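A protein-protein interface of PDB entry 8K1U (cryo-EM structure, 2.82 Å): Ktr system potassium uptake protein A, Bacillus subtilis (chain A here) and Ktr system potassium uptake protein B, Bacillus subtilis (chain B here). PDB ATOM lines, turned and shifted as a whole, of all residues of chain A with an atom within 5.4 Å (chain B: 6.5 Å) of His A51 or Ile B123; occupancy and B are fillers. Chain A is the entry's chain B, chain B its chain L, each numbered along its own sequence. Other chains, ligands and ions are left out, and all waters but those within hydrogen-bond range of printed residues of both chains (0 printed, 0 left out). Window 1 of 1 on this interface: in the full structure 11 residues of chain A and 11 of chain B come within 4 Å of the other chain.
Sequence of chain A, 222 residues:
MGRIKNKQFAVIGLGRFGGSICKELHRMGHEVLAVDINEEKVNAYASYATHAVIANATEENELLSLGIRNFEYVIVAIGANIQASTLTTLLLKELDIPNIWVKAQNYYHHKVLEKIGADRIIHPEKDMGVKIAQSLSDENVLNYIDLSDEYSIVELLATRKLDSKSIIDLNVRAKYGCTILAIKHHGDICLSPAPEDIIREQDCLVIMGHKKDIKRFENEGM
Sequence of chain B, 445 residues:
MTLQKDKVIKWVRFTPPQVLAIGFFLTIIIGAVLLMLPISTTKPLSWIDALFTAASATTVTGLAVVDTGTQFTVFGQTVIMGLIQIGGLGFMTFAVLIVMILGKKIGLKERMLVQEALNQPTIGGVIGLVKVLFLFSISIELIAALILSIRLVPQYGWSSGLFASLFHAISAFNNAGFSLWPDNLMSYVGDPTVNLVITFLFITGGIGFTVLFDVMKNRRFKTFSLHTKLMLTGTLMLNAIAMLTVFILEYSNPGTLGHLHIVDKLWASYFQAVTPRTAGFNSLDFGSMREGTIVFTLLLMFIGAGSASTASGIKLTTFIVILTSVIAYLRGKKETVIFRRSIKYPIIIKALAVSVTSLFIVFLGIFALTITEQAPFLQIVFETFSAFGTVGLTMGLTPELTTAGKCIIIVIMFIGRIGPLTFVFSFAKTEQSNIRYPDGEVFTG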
ATOM      1  N   VAL A  32      22.441 -17.194  14.470  1.00  0.00           N
ATOM      2  CA  VAL A  32      23.599 -16.674  15.186  1.00  0.00           C
ATOM      3  C   VAL A  32      23.171 -15.458  15.995  1.00  0.00           C
ATOM      4  O   VAL A  32      22.540 -14.540  15.459  1.00  0.00           O
ATOM      5  CB  VAL A  32      24.744 -16.308  14.224  1.00  0.00           C
ATOM      6  CG1 VAL A  32      26.001 -15.959  15.004  1.00  0.00           C
ATOM      7  CG2 VAL A  32      25.008 -17.446  13.254  1.00  0.00           C
ATOM      8  N   LEU A  33      23.515 -15.455  17.279  1.00  0.00           N
ATOM      9  CA  LEU A  33      23.316 -14.302  18.148  1.00  0.00           C
ATOM     10  C   LEU A  33      24.649 -13.584  18.313  1.00  0.00           C
ATOM     11  O   LEU A  33      25.621 -14.175  18.795  1.00  0.00           O
ATOM     12  CB  LEU A  33      22.761 -14.724  19.508  1.00  0.00           C
ATOM     13  CG  LEU A  33      22.626 -13.604  20.543  1.00  0.00           C
ATOM     14  CD1 LEU A  33      21.597 -12.578  20.095  1.00  0.00           C
ATOM     15  CD2 LEU A  33      22.275 -14.160  21.912  1.00  0.00           C
ATOM     16  N   ALA A  34      24.694 -12.317  17.911  1.00  0.00           N
ATOM     17  CA  ALA A  34      25.901 -11.508  18.000  1.00  0.00           C
ATOM     18  C   ALA A  34      25.781 -10.563  19.189  1.00  0.00           C
ATOM     19  O   ALA A  34      24.885  -9.712  19.221  1.00  0.00           O
ATOM     20  CB  ALA A  34      26.127 -10.725  16.709  1.00  0.00           C
ATOM     21  N   ALA A  49      24.089 -11.207  11.109  1.00  0.00           N
ATOM     22  CA  ALA A  49      23.680 -12.099  12.182  1.00  0.00           C
ATOM     23  C   ALA A  49      22.163 -12.155  12.237  1.00  0.00           C
ATOM     24  O   ALA A  49      21.476 -11.219  11.817  1.00  0.00           O
ATOM     25  CB  ALA A  49      24.241 -11.652  13.537  1.00  0.00           C
ATOM     26  N   THR A  50      21.645 -13.276  12.746  1.00  0.00           N
ATOM     27  CA  THR A  50      20.204 -13.408  12.938  1.00  0.00           C
ATOM     28  C   THR A  50      19.692 -12.399  13.956  1.00  0.00           C
ATOM     29  O   THR A  50      18.651 -11.763  13.745  1.00  0.00           O
ATOM     30  CB  THR A  50      19.865 -14.834  13.376  1.00  0.00           C
ATOM     31  OG1 THR A  50      20.343 -15.765  12.396  1.00  0.00           O
ATOM     32  CG2 THR A  50      18.361 -15.005  13.537  1.00  0.00           C
ATOM     33  N   HIS A  51      20.415 -12.228  15.059  1.00  0.00           N
ATOM     34  CA  HIS A  51      20.049 -11.271  16.094  1.00  0.00           C
ATOM     35  C   HIS A  51      21.319 -10.646  16.651  1.00  0.00           C
ATOM     36  O   HIS A  51      22.259 -11.362  17.009  1.00  0.00           O
ATOM     37  CB  HIS A  51      19.249 -11.947  17.213  1.00  0.00           C
ATOM     38  CG  HIS A  51      18.628 -10.987  18.180  1.00  0.00           C
ATOM     39  ND1 HIS A  51      18.023 -11.398  19.349  1.00  0.00           N
ATOM     40  CD2 HIS A  51      18.513  -9.639  18.152  1.00  0.00           C
ATOM     41  CE1 HIS A  51      17.566 -10.344  20.000  1.00  0.00           C
ATOM     42  NE2 HIS A  51      17.849  -9.264  19.294  1.00  0.00           N
ATOM     43  N   ALA A  52      21.346  -9.318  16.719  1.00  0.00           N
ATOM     44  CA  ALA A  52      22.487  -8.576  17.241  1.00  0.00           C
ATOM     45  C   ALA A  52      22.014  -7.714  18.401  1.00  0.00           C
ATOM     46  O   ALA A  52      21.058  -6.944  18.257  1.00  0.00           O
ATOM     47  CB  ALA A  52      23.128  -7.720  16.149  1.00  0.00           C
ATOM     48  N   VAL A  53      22.671  -7.853  19.552  1.00  0.00           N
ATOM     49  CA  VAL A  53      22.289  -7.154  20.773  1.00  0.00           C
ATOM     50  C   VAL A  53      23.506  -6.429  21.328  1.00  0.00           C
ATOM     51  O   VAL A  53      24.616  -6.973  21.331  1.00  0.00           O
ATOM     52  CB  VAL A  53      21.711  -8.117  21.837  1.00  0.00           C
ATOM     53  CG1 VAL A  53      21.103  -7.336  22.987  1.00  0.00           C
ATOM     54  CG2 VAL A  53      20.678  -9.056  21.231  1.00  0.00           C
ATOM     55  N   SER A  65      18.805 -11.826  29.848  1.00  0.00           N
ATOM     56  CA  SER A  65      17.841 -11.141  28.995  1.00  0.00           C
ATOM     57  C   SER A  65      17.972 -11.545  27.534  1.00  0.00           C
ATOM     58  O   SER A  65      17.058 -11.282  26.745  1.00  0.00           O
ATOM     59  CB  SER A  65      18.003  -9.625  29.132  1.00  0.00           C
ATOM     60  OG  SER A  65      17.820  -9.211  30.475  1.00  0.00           O
ATOM     61  N   LEU A  66      19.084 -12.174  27.154  1.00  0.00           N
ATOM     62  CA  LEU A  66      19.307 -12.602  25.781  1.00  0.00           C
ATOM     63  C   LEU A  66      18.739 -13.981  25.484  1.00  0.00           C
ATOM     64  O   LEU A  66      18.756 -14.402  24.322  1.00  0.00           O
ATOM     65  CB  LEU A  66      20.807 -12.604  25.465  1.00  0.00           C
ATOM     66  CG  LEU A  66      21.623 -11.399  25.930  1.00  0.00           C
ATOM     67  CD1 LEU A  66      23.089 -11.563  25.560  1.00  0.00           C
ATOM     68  CD2 LEU A  66      21.060 -10.116  25.354  1.00  0.00           C
ATOM     69  N   GLY A  67      18.232 -14.686  26.491  1.00  0.00           N
ATOM     70  CA  GLY A  67      17.865 -16.079  26.309  1.00  0.00           C
ATOM     71  C   GLY A  67      19.061 -16.959  26.026  1.00  0.00           C
ATOM     72  O   GLY A  67      18.981 -17.857  25.177  1.00  0.00           O
ATOM     73  N   LEU B 108      15.807 -19.159  17.342  1.00  0.00           N
ATOM     74  CA  LEU B 108      16.021 -17.747  17.642  1.00  0.00           C
ATOM     75  C   LEU B 108      15.100 -16.861  16.813  1.00  0.00           C
ATOM     76  O   LEU B 108      14.588 -15.852  17.311  1.00  0.00           O
ATOM     77  CB  LEU B 108      17.485 -17.374  17.405  1.00  0.00           C
ATOM     78  CG  LEU B 108      17.877 -15.919  17.669  1.00  0.00           C
ATOM     79  CD1 LEU B 108      17.577 -15.527  19.108  1.00  0.00           C
ATOM     80  CD2 LEU B 108      19.344 -15.689  17.344  1.00  0.00           C
ATOM     81  N   ARG B 111      11.723 -17.076  18.314  1.00  0.00           N
ATOM     82  CA  ARG B 111      11.653 -16.393  19.602  1.00  0.00           C
ATOM     83  C   ARG B 111      11.560 -14.881  19.430  1.00  0.00           C
ATOM     84  O   ARG B 111      10.998 -14.195  20.292  1.00  0.00           O
ATOM     85  CB  ARG B 111      12.865 -16.764  20.456  1.00  0.00           C
ATOM     86  CG  ARG B 111      12.709 -16.451  21.937  1.00  0.00           C
ATOM     87  CD  ARG B 111      13.880 -16.977  22.759  1.00  0.00           C
ATOM     88  NE  ARG B 111      14.018 -18.427  22.671  1.00  0.00           N
ATOM     89  CZ  ARG B 111      14.955 -19.051  21.971  1.00  0.00           C
ATOM     90  NH1 ARG B 111      15.869 -18.381  21.289  1.00  0.00           N
ATOM     91  NH2 ARG B 111      14.973 -20.380  21.952  1.00  0.00           N
ATOM     92  N   MET B 112      12.104 -14.346  18.334  1.00  0.00           N
ATOM     93  CA  MET B 112      11.991 -12.914  18.074  1.00  0.00           C
ATOM     94  C   MET B 112      10.567 -12.522  17.701  1.00  0.00           C
ATOM     95  O   MET B 112      10.157 -11.381  17.945  1.00  0.00           O
ATOM     96  CB  MET B 112      12.963 -12.500  16.970  1.00  0.00           C
ATOM     97  CG  MET B 112      14.428 -12.597  17.364  1.00  0.00           C
ATOM     98  SD  MET B 112      15.547 -12.262  15.990  1.00  0.00           S
ATOM     99  CE  MET B 112      15.074 -10.588  15.567  1.00  0.00           C
ATOM    100  N   GLN B 115       8.748 -11.948  20.944  1.00  0.00           N
ATOM    101  CA  GLN B 115       9.126 -10.674  21.551  1.00  0.00           C
ATOM    102  C   GLN B 115       8.341  -9.517  20.943  1.00  0.00           C
ATOM    103  O   GLN B 115       7.897  -8.613  21.661  1.00  0.00           O
ATOM    104  CB  GLN B 115      10.629 -10.446  21.384  1.00  0.00           C
ATOM    105  CG  GLN B 115      11.141  -9.155  21.999  1.00  0.00           C
ATOM    106  CD  GLN B 115      12.512  -8.765  21.480  1.00  0.00           C
ATOM    107  OE1 GLN B 115      12.950  -9.241  20.432  1.00  0.00           O
ATOM    108  NE2 GLN B 115      13.196  -7.894  22.211  1.00  0.00           N
ATOM    109  N   GLN B 120       7.651  -7.115  24.191  1.00  0.00           N
ATOM    110  CA  GLN B 120       8.719  -7.278  25.169  1.00  0.00           C
ATOM    111  C   GLN B 120       9.974  -6.541  24.710  1.00  0.00           C
ATOM    112  O   GLN B 120      10.221  -6.427  23.507  1.00  0.00           O
ATOM    113  CB  GLN B 120       9.037  -8.758  25.373  1.00  0.00           C
ATOM    114  CG  GLN B 120       9.081  -9.193  26.830  1.00  0.00           C
ATOM    115  CD  GLN B 120       7.754  -9.000  27.539  1.00  0.00           C
ATOM    116  OE1 GLN B 120       6.689  -9.188  26.952  1.00  0.00           O
ATOM    117  NE2 GLN B 120       7.814  -8.620  28.810  1.00  0.00           N
ATOM    118  N   PRO B 121      10.777  -6.016  25.639  1.00  0.00           N
ATOM    119  CA  PRO B 121      12.025  -5.354  25.239  1.00  0.00           C
ATOM    120  C   PRO B 121      13.165  -6.336  25.026  1.00  0.00           C
ATOM    121  O   PRO B 121      14.112  -6.047  24.285  1.00  0.00           O
ATOM    122  CB  PRO B 121      12.305  -4.409  26.413  1.00  0.00           C
ATOM    123  CG  PRO B 121      11.710  -5.108  27.586  1.00  0.00           C
ATOM    124  CD  PRO B 121      10.493  -5.838  27.074  1.00  0.00           C
ATOM    125  N   THR B 122      13.087  -7.499  25.669  1.00  0.00           N
ATOM    126  CA  THR B 122      14.126  -8.516  25.591  1.00  0.00           C
ATOM    127  C   THR B 122      13.494  -9.875  25.327  1.00  0.00           C
ATOM    128  O   THR B 122      12.305 -10.093  25.576  1.00  0.00           O
ATOM    129  CB  THR B 122      14.964  -8.578  26.879  1.00  0.00           C
ATOM    130  OG1 THR B 122      14.097  -8.689  28.014  1.00  0.00           O
ATOM    131  CG2 THR B 122      15.834  -7.335  27.022  1.00  0.00           C
ATOM    132  N   ILE B 123      14.312 -10.794  24.813  1.00  0.00           N
ATOM    133  CA  ILE B 123      13.868 -12.153  24.521  1.00  0.00           C
ATOM    134  C   ILE B 123      14.173 -13.058  25.707  1.00  0.00           C
ATOM    135  O   ILE B 123      14.070 -14.285  25.607  1.00  0.00           O
ATOM    136  CB  ILE B 123      14.525 -12.692  23.237  1.00  0.00           C
ATOM    137  CG1 ILE B 123      16.047 -12.558  23.318  1.00  0.00           C
ATOM    138  CG2 ILE B 123      13.985 -11.972  22.015  1.00  0.00           C
ATOM    139  CD1 ILE B 123      16.767 -13.038  22.076  1.00  0.00           C
ATOM    140  N   GLY B 124      14.552 -12.461  26.834  1.00  0.00           N
ATOM    141  CA  GLY B 124      14.871 -13.229  28.021  1.00  0.00           C
ATOM    142  C   GLY B 124      13.650 -13.778  28.726  1.00  0.00           C
ATOM    143  O   GLY B 124      12.878 -13.022  29.324  1.00  0.00           O
ATOM    144  N   GLY B 125      13.472 -15.094  28.672  1.00  0.00           N
ATOM    145  CA  GLY B 125      12.336 -15.734  29.312  1.00  0.00           C
ATOM    146  C   GLY B 125      10.992 -15.368  28.721  1.00  0.00           C
ATOM    147  O   GLY B 125      10.027 -15.163  29.469  1.00  0.00           O
ATOM    148  N   VAL B 126      10.903 -15.279  27.395  1.00  0.00           N
ATOM    149  CA  VAL B 126       9.644 -14.950  26.738  1.00  0.00           C
ATOM    150  C   VAL B 126       8.890 -16.196  26.273  1.00  0.00           C
ATOM    151  O   VAL B 126       7.659 -16.144  26.132  1.00  0.00           O
ATOM    152  CB  VAL B 126       9.881 -13.972  25.563  1.00  0.00           C
ATOM    153  CG1 VAL B 126      10.481 -14.683  24.354  1.00  0.00           C
ATOM    154  CG2 VAL B 126       8.599 -13.232  25.193  1.00  0.00           C
ATOM    155  N   ILE B 127       9.585 -17.315  26.048  1.00  0.00           N
ATOM    156  CA  ILE B 127       8.904 -18.559  25.705  1.00  0.00           C
ATOM    157  C   ILE B 127       8.160 -19.108  26.916  1.00  0.00           C
ATOM    158  O   ILE B 127       7.019 -19.573  26.803  1.00  0.00           O
ATOM    159  CB  ILE B 127       9.910 -19.575  25.136  1.00  0.00           C
ATOM    160  CG1 ILE B 127      10.508 -19.050  23.830  1.00  0.00           C
ATOM    161  CG2 ILE B 127       9.249 -20.928  24.909  1.00  0.00           C
ATOM    162  CD1 ILE B 127       9.471 -18.733  22.771  1.00  0.00           C
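The backbone NH (N) of Thr A50 sits at hydrogen-bond distance from the backbone carbonyl oxygen (O) of Val A32 (3.1 Å). O of Val A32 lies within hydrogen-bond range of N of His A51 (3.2 Å). The backbone NH (N) of Ala A34 lies within hydrogen-bond range of the backbone carbonyl oxygen (O) of His A51, at 2.8 Å. NE2 of Gln B115 sits close to N of Thr B122, at 3.5 Å.
The backbone NH (N) of Ile B123 is in hydrogen-bond range of the backbone carbonyl oxygen (O) of Ser A65, at 3.4 Å. The backbone NH (N) of Gly B124 sits at hydrogen-bond distance from the backbone carbonyl oxygen (O) of Ser A65.
Hydrophobic or aromatic side chains of chain A within 4 Å of the printed part of chain B: His A51. Of the 12 printed residues of chain B, 5 touch a printed residue of chain A. Hydrophobic or aromatic side chains of chain B that line the printed part of chain A: Leu B108, Met B112 and Ile B123. Along chain B the printed residues that touch a printed residue of chain A span positions 108 to 124. Among the printed residues, 11 pairs touch across the chains. Among the printed residues, no Asp or Glu carboxylate lies within 4 Å of a Lys or Arg side-chain nitrogen of the other chain.
Val A32 touches Leu B108 (O to CD2, 3.9 Å). Leu B108 touches Thr A50. Met B112 touches Thr A50 (SD to O, 3.9 Å). His A51 touches Leu B108 (CB to CD2, 3.7 Å). SD of Met B112 touches CB of His A51, at 3.9 Å. ND1 of His A51 touches CD1 of Ile B123, at 3.4 Å. O of Ser A65 touches CB of Thr B122 (3.4 Å). Leu A66 touches Ile B123. N of Gly A67 touches CA of Gly B124, 3.97 Å away.
Printed residues of chain B within 4 Å of Val A32: Leu B108. His A51 touches just these residues of chain B: Leu B108, Met B112 and Ile B123. Printed residues of chain B within 4 Å of Leu A66: Ile B123. Of the printed residues of chain A, Leu B108 touches Val A32 (3.9 Å), Thr A50 (3.99 Å) and His A51 (3.7 Å). Of the printed residues of chain A, Ile B123 touches His A51 (3.4 Å), Ser A65 (3.4 Å) and Leu A66 (3.3 Å). Val B126 touches none of the printed residues of chain A. The nearest residue of chain A that does not touch Ile B123 is Gly A67 (4.3 Å). The nearest printed residue of chain A that does not touch Gly B124 is Leu A66 (4.4 Å).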
